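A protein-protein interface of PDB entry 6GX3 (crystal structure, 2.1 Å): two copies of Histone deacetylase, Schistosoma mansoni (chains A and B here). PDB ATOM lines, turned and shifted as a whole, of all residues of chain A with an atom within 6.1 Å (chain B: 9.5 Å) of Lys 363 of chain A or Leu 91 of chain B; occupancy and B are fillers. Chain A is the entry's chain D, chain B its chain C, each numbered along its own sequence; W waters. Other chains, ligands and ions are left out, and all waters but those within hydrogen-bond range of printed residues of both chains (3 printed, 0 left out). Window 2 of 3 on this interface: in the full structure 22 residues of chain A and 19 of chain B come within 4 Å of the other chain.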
ATOM      1  N   SER A   3     -13.757  14.704 -26.752  1.00  0.00           N
ATOM      2  CA  SER A   3     -12.888  15.861 -26.615  1.00  0.00           C
ATOM      3  C   SER A   3     -11.500  15.567 -27.181  1.00  0.00           C
ATOM      4  O   SER A   3     -10.989  14.450 -27.055  1.00  0.00           O
ATOM      5  CB  SER A   3     -12.783  16.280 -25.148  1.00  0.00           C
ATOM      6  OG  SER A   3     -11.947  17.417 -25.003  1.00  0.00           O
ATOM      7  N   VAL A   4     -10.901  16.567 -27.817  1.00  0.00           N
ATOM      8  CA  VAL A   4      -9.532  16.450 -28.286  1.00  0.00           C
ATOM      9  C   VAL A   4      -8.677  17.440 -27.509  1.00  0.00           C
ATOM     10  O   VAL A   4      -8.955  18.642 -27.491  1.00  0.00           O
ATOM     11  CB  VAL A   4      -9.407  16.708 -29.805  1.00  0.00           C
ATOM     12  CG1 VAL A   4      -7.945  16.585 -30.257  1.00  0.00           C
ATOM     13  CG2 VAL A   4     -10.269  15.730 -30.586  1.00  0.00           C
ATOM     14  N   ILE A  39      -7.948  26.146 -32.335  1.00  0.00           N
ATOM     15  CA  ILE A  39      -7.731  26.147 -30.886  1.00  0.00           C
ATOM     16  C   ILE A  39      -9.040  26.189 -30.065  1.00  0.00           C
ATOM     17  O   ILE A  39      -9.131  25.521 -29.034  1.00  0.00           O
ATOM     18  CB  ILE A  39      -6.789  27.314 -30.472  1.00  0.00           C
ATOM     19  CG1 ILE A  39      -5.343  26.998 -30.867  1.00  0.00           C
ATOM     20  CG2 ILE A  39      -6.841  27.583 -28.976  1.00  0.00           C
ATOM     21  CD1 ILE A  39      -4.815  25.691 -30.269  1.00  0.00           C
ATOM     22  N   PRO A  40     -10.064  26.948 -30.515  1.00  0.00           N
ATOM     23  CA  PRO A  40     -11.326  26.860 -29.767  1.00  0.00           C
ATOM     24  C   PRO A  40     -11.986  25.479 -29.801  1.00  0.00           C
ATOM     25  O   PRO A  40     -12.827  25.184 -28.950  1.00  0.00           O
ATOM     26  CB  PRO A  40     -12.209  27.893 -30.465  1.00  0.00           C
ATOM     27  CG  PRO A  40     -11.243  28.903 -30.964  1.00  0.00           C
ATOM     28  CD  PRO A  40     -10.080  28.089 -31.449  1.00  0.00           C
ATOM     29  N   GLU A  41     -11.614  24.651 -30.767  1.00  0.00           N
ATOM     30  CA  GLU A  41     -12.134  23.284 -30.859  1.00  0.00           C
ATOM     31  C   GLU A  41     -11.411  22.292 -29.927  1.00  0.00           C
ATOM     32  O   GLU A  41     -11.885  21.179 -29.706  1.00  0.00           O
ATOM     33  CB  GLU A  41     -12.036  22.789 -32.304  1.00  0.00           C
ATOM     34  CG  GLU A  41     -12.699  23.705 -33.321  1.00  0.00           C
ATOM     35  CD  GLU A  41     -14.200  23.802 -33.123  1.00  0.00           C
ATOM     36  OE1 GLU A  41     -14.841  22.747 -32.951  1.00  0.00           O
ATOM     37  OE2 GLU A  41     -14.735  24.933 -33.126  1.00  0.00           O
ATOM     38  N   LEU A  42     -10.275  22.696 -29.372  1.00  0.00           N
ATOM     39  CA  LEU A  42      -9.467  21.773 -28.576  1.00  0.00           C
ATOM     40  C   LEU A  42      -9.463  22.145 -27.101  1.00  0.00           C
ATOM     41  O   LEU A  42      -9.568  23.308 -26.744  1.00  0.00           O
ATOM     42  CB  LEU A  42      -8.029  21.733 -29.097  1.00  0.00           C
ATOM     43  CG  LEU A  42      -7.849  21.516 -30.604  1.00  0.00           C
ATOM     44  CD1 LEU A  42      -6.679  22.333 -31.138  1.00  0.00           C
ATOM     45  CD2 LEU A  42      -7.637  20.060 -30.921  1.00  0.00           C
ATOM     46  N   SER A  43      -9.331  21.138 -26.256  1.00  0.00           N
ATOM     47  CA  SER A  43      -9.196  21.323 -24.822  1.00  0.00           C
ATOM     48  C   SER A  43      -7.719  21.513 -24.448  1.00  0.00           C
ATOM     49  O   SER A  43      -6.885  20.651 -24.750  1.00  0.00           O
ATOM     50  CB  SER A  43      -9.803  20.110 -24.108  1.00  0.00           C
ATOM     51  OG  SER A  43      -9.349  19.993 -22.776  1.00  0.00           O
ATOM     52  N   ARG A  44      -7.380  22.636 -23.815  1.00  0.00           N
ATOM     53  CA  ARG A  44      -5.998  22.833 -23.380  1.00  0.00           C
ATOM     54  C   ARG A  44      -5.626  21.806 -22.317  1.00  0.00           C
ATOM     55  O   ARG A  44      -6.325  21.676 -21.304  1.00  0.00           O
ATOM     56  CB  ARG A  44      -5.751  24.237 -22.823  1.00  0.00           C
ATOM     57  CG  ARG A  44      -4.445  24.314 -21.993  1.00  0.00           C
ATOM     58  CD  ARG A  44      -3.841  25.718 -21.923  1.00  0.00           C
ATOM     59  NE  ARG A  44      -3.876  26.292 -20.573  1.00  0.00           N
ATOM     60  CZ  ARG A  44      -2.865  26.259 -19.699  1.00  0.00           C
ATOM     61  NH1 ARG A  44      -1.706  25.676 -20.011  1.00  0.00           N
ATOM     62  NH2 ARG A  44      -3.013  26.818 -18.503  1.00  0.00           N
ATOM     63  N   THR A 358      -7.932  15.123 -36.659  1.00  0.00           N
ATOM     64  CA  THR A 358      -8.257  14.565 -35.361  1.00  0.00           C
ATOM     65  C   THR A 358      -9.568  15.186 -34.874  1.00  0.00           C
ATOM     66  O   THR A 358     -10.481  14.472 -34.479  1.00  0.00           O
ATOM     67  CB  THR A 358      -7.102  14.802 -34.356  1.00  0.00           C
ATOM     68  OG1 THR A 358      -5.897  14.195 -34.858  1.00  0.00           O
ATOM     69  CG2 THR A 358      -7.427  14.210 -32.996  1.00  0.00           C
ATOM     70  N   ILE A 359      -9.666  16.512 -34.924  1.00  0.00           N
ATOM     71  CA  ILE A 359     -10.893  17.205 -34.560  1.00  0.00           C
ATOM     72  C   ILE A 359     -12.103  16.676 -35.339  1.00  0.00           C
ATOM     73  O   ILE A 359     -13.156  16.414 -34.749  1.00  0.00           O
ATOM     74  CB  ILE A 359     -10.772  18.718 -34.794  1.00  0.00           C
ATOM     75  CG1 ILE A 359      -9.843  19.341 -33.750  1.00  0.00           C
ATOM     76  CG2 ILE A 359     -12.149  19.381 -34.750  1.00  0.00           C
ATOM     77  CD1 ILE A 359      -9.445  20.766 -34.074  1.00  0.00           C
ATOM     78  N   GLU A 360     -11.949  16.503 -36.651  1.00  0.00           N
ATOM     79  CA  GLU A 360     -13.021  15.953 -37.491  1.00  0.00           C
ATOM     80  C   GLU A 360     -13.413  14.541 -37.082  1.00  0.00           C
ATOM     81  O   GLU A 360     -14.588  14.244 -36.884  1.00  0.00           O
ATOM     82  CB  GLU A 360     -12.616  15.930 -38.968  1.00  0.00           C
ATOM     83  CG  GLU A 360     -12.669  17.267 -39.671  1.00  0.00           C
ATOM     84  CD  GLU A 360     -12.868  17.118 -41.177  1.00  0.00           C
ATOM     85  OE1 GLU A 360     -12.902  15.966 -41.664  1.00  0.00           O
ATOM     86  OE2 GLU A 360     -13.000  18.149 -41.871  1.00  0.00           O
ATOM     87  N   GLU A 361     -12.414  13.671 -36.981  1.00  0.00           N
ATOM     88  CA  GLU A 361     -12.634  12.260 -36.705  1.00  0.00           C
ATOM     89  C   GLU A 361     -13.188  11.996 -35.316  1.00  0.00           C
ATOM     90  O   GLU A 361     -13.846  10.985 -35.097  1.00  0.00           O
ATOM     91  CB  GLU A 361     -11.333  11.476 -36.875  1.00  0.00           C
ATOM     92  CG  GLU A 361     -10.886  11.330 -38.306  1.00  0.00           C
ATOM     93  CD  GLU A 361     -11.933  10.649 -39.152  1.00  0.00           C
ATOM     94  OE1 GLU A 361     -12.292   9.494 -38.838  1.00  0.00           O
ATOM     95  OE2 GLU A 361     -12.404  11.277 -40.123  1.00  0.00           O
ATOM     96  N   VAL A 362     -12.917  12.885 -34.369  1.00  0.00           N
ATOM     97  CA  VAL A 362     -13.368  12.644 -33.004  1.00  0.00           C
ATOM     98  C   VAL A 362     -14.699  13.332 -32.709  1.00  0.00           C
ATOM     99  O   VAL A 362     -15.610  12.706 -32.181  1.00  0.00           O
ATOM    100  CB  VAL A 362     -12.321  13.101 -31.982  1.00  0.00           C
ATOM    101  CG1 VAL A 362     -12.848  12.911 -30.554  1.00  0.00           C
ATOM    102  CG2 VAL A 362     -11.014  12.327 -32.186  1.00  0.00           C
ATOM    103  N   LYS A 363     -14.816  14.610 -33.061  1.00  0.00           N
ATOM    104  CA  LYS A 363     -16.019  15.380 -32.763  1.00  0.00           C
ATOM    105  C   LYS A 363     -17.095  15.257 -33.840  1.00  0.00           C
ATOM    106  O   LYS A 363     -18.219  15.686 -33.637  1.00  0.00           O
ATOM    107  CB  LYS A 363     -15.670  16.853 -32.571  1.00  0.00           C
ATOM    108  CG  LYS A 363     -14.621  17.078 -31.503  1.00  0.00           C
ATOM    109  CD  LYS A 363     -14.214  18.538 -31.406  1.00  0.00           C
ATOM    110  CE  LYS A 363     -15.358  19.410 -30.910  1.00  0.00           C
ATOM    111  NZ  LYS A 363     -14.913  20.820 -30.696  1.00  0.00           N
ATOM    112  N   GLY A 364     -16.743  14.679 -34.985  1.00  0.00           N
ATOM    113  CA  GLY A 364     -17.680  14.531 -36.087  1.00  0.00           C
ATOM    114  C   GLY A 364     -17.919  15.851 -36.798  1.00  0.00           C
ATOM    115  O   GLY A 364     -18.673  15.934 -37.765  1.00  0.00           O
ATOM    116  N   LYS A 365     -17.248  16.884 -36.307  1.00  0.00           N
ATOM    117  CA  LYS A 365     -17.420  18.250 -36.774  1.00  0.00           C
ATOM    118  C   LYS A 365     -16.489  18.490 -37.954  1.00  0.00           C
ATOM    119  O   LYS A 365     -15.275  18.327 -37.829  1.00  0.00           O
ATOM    120  CB  LYS A 365     -17.120  19.215 -35.625  1.00  0.00           C
ATOM    121  CG  LYS A 365     -17.839  20.546 -35.653  1.00  0.00           C
ATOM    122  CD  LYS A 365     -17.661  21.248 -34.308  1.00  0.00           C
ATOM    123  CE  LYS A 365     -18.002  22.730 -34.377  1.00  0.00           C
ATOM    124  NZ  LYS A 365     -17.702  23.422 -33.082  1.00  0.00           N
ATOM    125  N   ALA B  71     -17.413  32.680 -16.761  1.00  0.00           N
ATOM    126  CA  ALA B  71     -17.154  31.241 -16.804  1.00  0.00           C
ATOM    127  C   ALA B  71     -17.189  30.634 -15.402  1.00  0.00           C
ATOM    128  O   ALA B  71     -17.749  29.555 -15.184  1.00  0.00           O
ATOM    129  CB  ALA B  71     -15.812  30.966 -17.451  1.00  0.00           C
ATOM    130  N   LEU B  78     -23.325  25.073 -12.750  1.00  0.00           N
ATOM    131  CA  LEU B  78     -23.287  23.695 -13.241  1.00  0.00           C
ATOM    132  C   LEU B  78     -23.136  22.656 -12.120  1.00  0.00           C
ATOM    133  O   LEU B  78     -23.851  21.656 -12.089  1.00  0.00           O
ATOM    134  CB  LEU B  78     -22.151  23.530 -14.259  1.00  0.00           C
ATOM    135  CG  LEU B  78     -22.291  24.297 -15.579  1.00  0.00           C
ATOM    136  CD1 LEU B  78     -21.027  24.168 -16.413  1.00  0.00           C
ATOM    137  CD2 LEU B  78     -23.503  23.832 -16.378  1.00  0.00           C
ATOM    138  N   LEU B  85     -21.663  18.322 -17.859  1.00  0.00           N
ATOM    139  CA  LEU B  85     -21.410  19.432 -18.778  1.00  0.00           C
ATOM    140  C   LEU B  85     -21.569  19.001 -20.228  1.00  0.00           C
ATOM    141  O   LEU B  85     -21.312  17.850 -20.563  1.00  0.00           O
ATOM    142  CB  LEU B  85     -20.000  19.996 -18.576  1.00  0.00           C
ATOM    143  CG  LEU B  85     -19.786  21.129 -17.576  1.00  0.00           C
ATOM    144  CD1 LEU B  85     -19.978  20.642 -16.142  1.00  0.00           C
ATOM    145  CD2 LEU B  85     -18.401  21.753 -17.766  1.00  0.00           C
ATOM    146  N   THR B  86     -21.985  19.926 -21.087  1.00  0.00           N
ATOM    147  CA  THR B  86     -21.947  19.679 -22.524  1.00  0.00           C
ATOM    148  C   THR B  86     -20.500  19.766 -23.008  1.00  0.00           C
ATOM    149  O   THR B  86     -19.649  20.335 -22.321  1.00  0.00           O
ATOM    150  CB  THR B  86     -22.811  20.680 -23.311  1.00  0.00           C
ATOM    151  OG1 THR B  86     -22.130  21.940 -23.410  1.00  0.00           O
ATOM    152  CG2 THR B  86     -24.171  20.866 -22.639  1.00  0.00           C
ATOM    153  N   ALA B  87     -20.227  19.206 -24.182  1.00  0.00           N
ATOM    154  CA  ALA B  87     -18.893  19.257 -24.776  1.00  0.00           C
ATOM    155  C   ALA B  87     -18.343  20.682 -24.821  1.00  0.00           C
ATOM    156  O   ALA B  87     -17.159  20.894 -24.572  1.00  0.00           O
ATOM    157  CB  ALA B  87     -18.905  18.647 -26.188  1.00  0.00           C
ATOM    158  N   ASP B  88     -19.197  21.662 -25.119  1.00  0.00           N
ATOM    159  CA  ASP B  88     -18.725  23.041 -25.242  1.00  0.00           C
ATOM    160  C   ASP B  88     -18.577  23.772 -23.895  1.00  0.00           C
ATOM    161  O   ASP B  88     -17.682  24.606 -23.732  1.00  0.00           O
ATOM    162  CB  ASP B  88     -19.642  23.820 -26.171  1.00  0.00           C
ATOM    163  CG  ASP B  88     -19.605  23.286 -27.590  1.00  0.00           C
ATOM    164  OD1 ASP B  88     -18.559  22.722 -27.991  1.00  0.00           O
ATOM    165  OD2 ASP B  88     -20.620  23.417 -28.300  1.00  0.00           O
ATOM    166  N   ASP B  89     -19.430  23.470 -22.923  1.00  0.00           N
ATOM    167  CA  ASP B  89     -19.184  24.000 -21.586  1.00  0.00           C
ATOM    168  C   ASP B  89     -17.834  23.474 -21.081  1.00  0.00           C
ATOM    169  O   ASP B  89     -17.073  24.198 -20.427  1.00  0.00           O
ATOM    170  CB  ASP B  89     -20.308  23.624 -20.617  1.00  0.00           C
ATOM    171  CG  ASP B  89     -21.614  24.356 -20.910  1.00  0.00           C
ATOM    172  OD1 ASP B  89     -21.577  25.523 -21.373  1.00  0.00           O
ATOM    173  OD2 ASP B  89     -22.683  23.754 -20.668  1.00  0.00           O
ATOM    174  N   GLU B  90     -17.538  22.216 -21.405  1.00  0.00           N
ATOM    175  CA  GLU B  90     -16.250  21.623 -21.051  1.00  0.00           C
ATOM    176  C   GLU B  90     -15.090  22.385 -21.685  1.00  0.00           C
ATOM    177  O   GLU B  90     -14.100  22.690 -21.006  1.00  0.00           O
ATOM    178  CB  GLU B  90     -16.189  20.158 -21.473  1.00  0.00           C
ATOM    179  CG  GLU B  90     -17.181  19.254 -20.764  1.00  0.00           C
ATOM    180  CD  GLU B  90     -16.681  18.759 -19.428  1.00  0.00           C
ATOM    181  OE1 GLU B  90     -15.562  19.139 -19.021  1.00  0.00           O
ATOM    182  OE2 GLU B  90     -17.410  17.978 -18.784  1.00  0.00           O
ATOM    183  N   LEU B  91     -15.213  22.689 -22.978  1.00  0.00           N
ATOM    184  CA  LEU B  91     -14.183  23.450 -23.681  1.00  0.00           C
ATOM    185  C   LEU B  91     -14.070  24.851 -23.097  1.00  0.00           C
ATOM    186  O   LEU B  91     -12.975  25.403 -22.994  1.00  0.00           O
ATOM    187  CB  LEU B  91     -14.474  23.532 -25.184  1.00  0.00           C
ATOM    188  CG  LEU B  91     -14.236  22.297 -26.053  1.00  0.00           C
ATOM    189  CD1 LEU B  91     -14.926  22.459 -27.396  1.00  0.00           C
ATOM    190  CD2 LEU B  91     -12.751  22.050 -26.252  1.00  0.00           C
ATOM    191  N   LEU B  92     -15.208  25.419 -22.719  1.00  0.00           N
ATOM    192  CA  LEU B  92     -15.231  26.732 -22.089  1.00  0.00           C
ATOM    193  C   LEU B  92     -14.443  26.713 -20.778  1.00  0.00           C
ATOM    194  O   LEU B  92     -13.583  27.564 -20.553  1.00  0.00           O
ATOM    195  CB  LEU B  92     -16.670  27.188 -21.841  1.00  0.00           C
ATOM    196  CG  LEU B  92     -16.824  28.477 -21.019  1.00  0.00           C
ATOM    197  CD1 LEU B  92     -16.307  29.697 -21.785  1.00  0.00           C
ATOM    198  CD2 LEU B  92     -18.269  28.678 -20.561  1.00  0.00           C
ATOM    199  N   MET B  93     -14.728  25.731 -19.923  1.00  0.00           N
ATOM    200  CA  MET B  93     -14.002  25.599 -18.667  1.00  0.00           C
ATOM    201  C   MET B  93     -12.505  25.328 -18.918  1.00  0.00           C
ATOM    202  O   MET B  93     -11.655  25.937 -18.277  1.00  0.00           O
ATOM    203  CB  MET B  93     -14.629  24.500 -17.795  1.00  0.00           C
ATOM    204  CG  MET B  93     -16.075  24.827 -17.400  1.00  0.00           C
ATOM    205  SD  MET B  93     -16.301  26.566 -16.877  1.00  0.00           S
ATOM    206  CE  MET B  93     -17.961  26.891 -17.502  1.00  0.00           C
ATOM    207  N   ASP B  94     -12.191  24.444 -19.860  1.00  0.00           N
ATOM    208  CA  ASP B  94     -10.793  24.123 -20.160  1.00  0.00           C
ATOM    209  C   ASP B  94     -10.010  25.361 -20.622  1.00  0.00           C
ATOM    210  O   ASP B  94      -8.836  25.526 -20.290  1.00  0.00           O
ATOM    211  CB  ASP B  94     -10.704  23.023 -21.229  1.00  0.00           C
ATOM    212  CG  ASP B  94     -11.173  21.663 -20.718  1.00  0.00           C
ATOM    213  OD1 ASP B  94     -11.295  21.479 -19.488  1.00  0.00           O
ATOM    214  OD2 ASP B  94     -11.425  20.771 -21.549  1.00  0.00           O
ATOM    215  N   SER B  95     -10.665  26.244 -21.365  1.00  0.00           N
ATOM    216  CA  SER B  95      -9.983  27.441 -21.827  1.00  0.00           C
ATOM    217  C   SER B  95      -9.595  28.376 -20.676  1.00  0.00           C
ATOM    218  O   SER B  95      -8.783  29.280 -20.870  1.00  0.00           O
ATOM    219  CB  SER B  95     -10.848  28.197 -22.839  1.00  0.00           C
ATOM    220  OG  SER B  95     -11.879  28.938 -22.204  1.00  0.00           O
ATOM    221  N   PHE B  96     -10.172  28.181 -19.486  1.00  0.00           N
ATOM    222  CA  PHE B  96      -9.841  29.062 -18.360  1.00  0.00           C
ATOM    223  C   PHE B  96      -9.081  28.323 -17.267  1.00  0.00           C
ATOM    224  O   PHE B  96      -8.914  28.832 -16.153  1.00  0.00           O
ATOM    225  CB  PHE B  96     -11.105  29.708 -17.782  1.00  0.00           C
ATOM    226  CG  PHE B  96     -11.778  30.656 -18.739  1.00  0.00           C
ATOM    227  CD1 PHE B  96     -11.181  31.856 -19.073  1.00  0.00           C
ATOM    228  CD2 PHE B  96     -12.989  30.329 -19.325  1.00  0.00           C
ATOM    229  CE1 PHE B  96     -11.784  32.718 -19.955  1.00  0.00           C
ATOM    230  CE2 PHE B  96     -13.598  31.187 -20.211  1.00  0.00           C
ATOM    231  CZ  PHE B  96     -12.994  32.384 -20.529  1.00  0.00           C
ATOM    232  N   SER B  97      -8.612  27.129 -17.613  1.00  0.00           N
ATOM    233  CA  SER B  97      -7.957  26.228 -16.673  1.00  0.00           C
ATOM    234  C   SER B  97      -8.868  25.955 -15.486  1.00  0.00           C
ATOM    235  O   SER B  97      -8.400  25.736 -14.373  1.00  0.00           O
ATOM    236  CB  SER B  97      -6.620  26.793 -16.196  1.00  0.00           C
ATOM    237  OG  SER B  97      -5.788  27.092 -17.295  1.00  0.00           O
ATOM    238  N   LEU B  98     -10.176  25.975 -15.727  1.00  0.00           N
ATOM    239  CA  LEU B  98     -11.134  25.598 -14.693  1.00  0.00           C
ATOM    240  C   LEU B  98     -11.258  24.077 -14.689  1.00  0.00           C
ATOM    241  O   LEU B  98     -12.325  23.516 -14.925  1.00  0.00           O
ATOM    242  CB  LEU B  98     -12.477  26.296 -14.925  1.00  0.00           C
ATOM    243  CG  LEU B  98     -12.333  27.801 -14.657  1.00  0.00           C
ATOM    244  CD1 LEU B  98     -13.565  28.598 -15.102  1.00  0.00           C
ATOM    245  CD2 LEU B  98     -12.020  28.033 -13.171  1.00  0.00           C
ATOM    246  N   ASN B  99     -10.126  23.429 -14.430  1.00  0.00           N
ATOM    247  CA  ASN B  99      -9.988  21.978 -14.503  1.00  0.00           C
ATOM    248  C   ASN B  99      -8.794  21.516 -13.661  1.00  0.00           C
ATOM    249  O   ASN B  99      -8.108  22.341 -13.063  1.00  0.00           O
ATOM    250  CB  ASN B  99      -9.829  21.532 -15.962  1.00  0.00           C
ATOM    251  CG  ASN B  99      -8.718  22.286 -16.692  1.00  0.00           C
ATOM    252  OD1 ASN B  99      -7.786  22.807 -16.071  1.00  0.00           O
ATOM    253  ND2 ASN B  99      -8.809  22.337 -18.019  1.00  0.00           N
HETATM  254  O   HOH W   1     -13.192  18.871 -22.538  1.00  0.00           O
HETATM  255  O   HOH W   2      -7.093  23.640 -19.697  1.00  0.00           O
HETATM  256  O   HOH W   3      -9.821  24.802 -24.140  1.00  0.00           O
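Water W2 lies within hydrogen-bond range of O of Asp 94 of chain B, O of Arg 44 of chain A and ND2 of Asn 99 of chain B. Water W1 bridges OD2 of Asp 94 of chain B (2.8 Å) and OG of Ser 3 of chain A (3.1 Å). Water W3 lies within hydrogen-bond range of O of Leu 42 of chain A (3.0 Å), N of Ser 95 of chain B (3.2 Å), N of Arg 44 of chain A (3.3 Å) and O of Leu 91 of chain B (3.4 Å).
No position is printed for both chains.
The side-chain amide nitrogen (ND2) of Asn 99 of chain B lies within hydrogen-bond range of the side-chain carboxylate (OD1) of Asp 94 of chain B. O of Ser 97 of chain B lies close to OD1 of Asn 99 of chain B. N of Ser 43 of chain A is in hydrogen-bond range of O of Val 4 of chain A. The side-chain carboxylate (OE1) of Glu 41 of chain A is in salt-bridge range of the side-chain amino group (NZ) of Lys 363 of chain A, at 3.0 Å. The side-chain carboxylate of Glu 41 of chain A is in salt-bridge range of the side-chain amino group of Lys 365 of chain A.
The side-chain hydroxyl (OG) of Ser 43 of chain A lies within hydrogen-bond range of the side-chain carboxylate (OD2) of Asp 94 of chain B, 2.5 Å away. The side-chain hydroxyl (OG) of Ser 97 of chain B lies within hydrogen-bond range of the guanidinium group (NH2) of Arg 44 of chain A (3.0 Å).
Along chain A the printed residues that touch a printed residue of chain B span positions 40 to 363. Printed residues of chain B that touch a printed residue of chain A: Leu 91, Asp 94 and Ser 97. Hydrophobic or aromatic side chains of chain B that line the printed part of chain A: Leu 91. Among the printed residues, no Asp or Glu carboxylate lies within 4 Å of a Lys or Arg side-chain nitrogen of the other chain.
Among the printed residues, pairs that only touch across the chains: Pro 40 of chain A with Leu 91 of chain B, Glu 41 of chain A with Leu 91 of chain B, Leu 42 of chain A with Leu 91 of chain B, Ser 43 of chain A with Leu 91 of chain B and Lys 363 of chain A with Leu 91 of chain B.
Of the printed residues of chain B, Pro 40 of chain A touches Leu 91 (3.8 Å). Glu 41 of chain A touches one residue of chain B. Of the printed residues of chain B, Leu 42 of chain A touches Leu 91 (3.4 Å). Val 362 of chain A touches none of the printed residues of chain B. No residue of chain B comes within 4 Å of Gly 364 of chain A. No residue of chain B comes within 4 Å of Lys 365 of chain A. Ala 71 of chain B touches none of the printed residues of chain A. Of chain A, only Pro 40 (3.8 Å), Glu 41 (3.7 Å), Leu 42 (3.4 Å), Ser 43 (3.5 Å) and Lys 363 (3.7 Å) come within 4 Å of Leu 91 of chain B. Of the printed residues of chain A, Ser 97 of chain B touches Arg 44 (3.0 Å).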
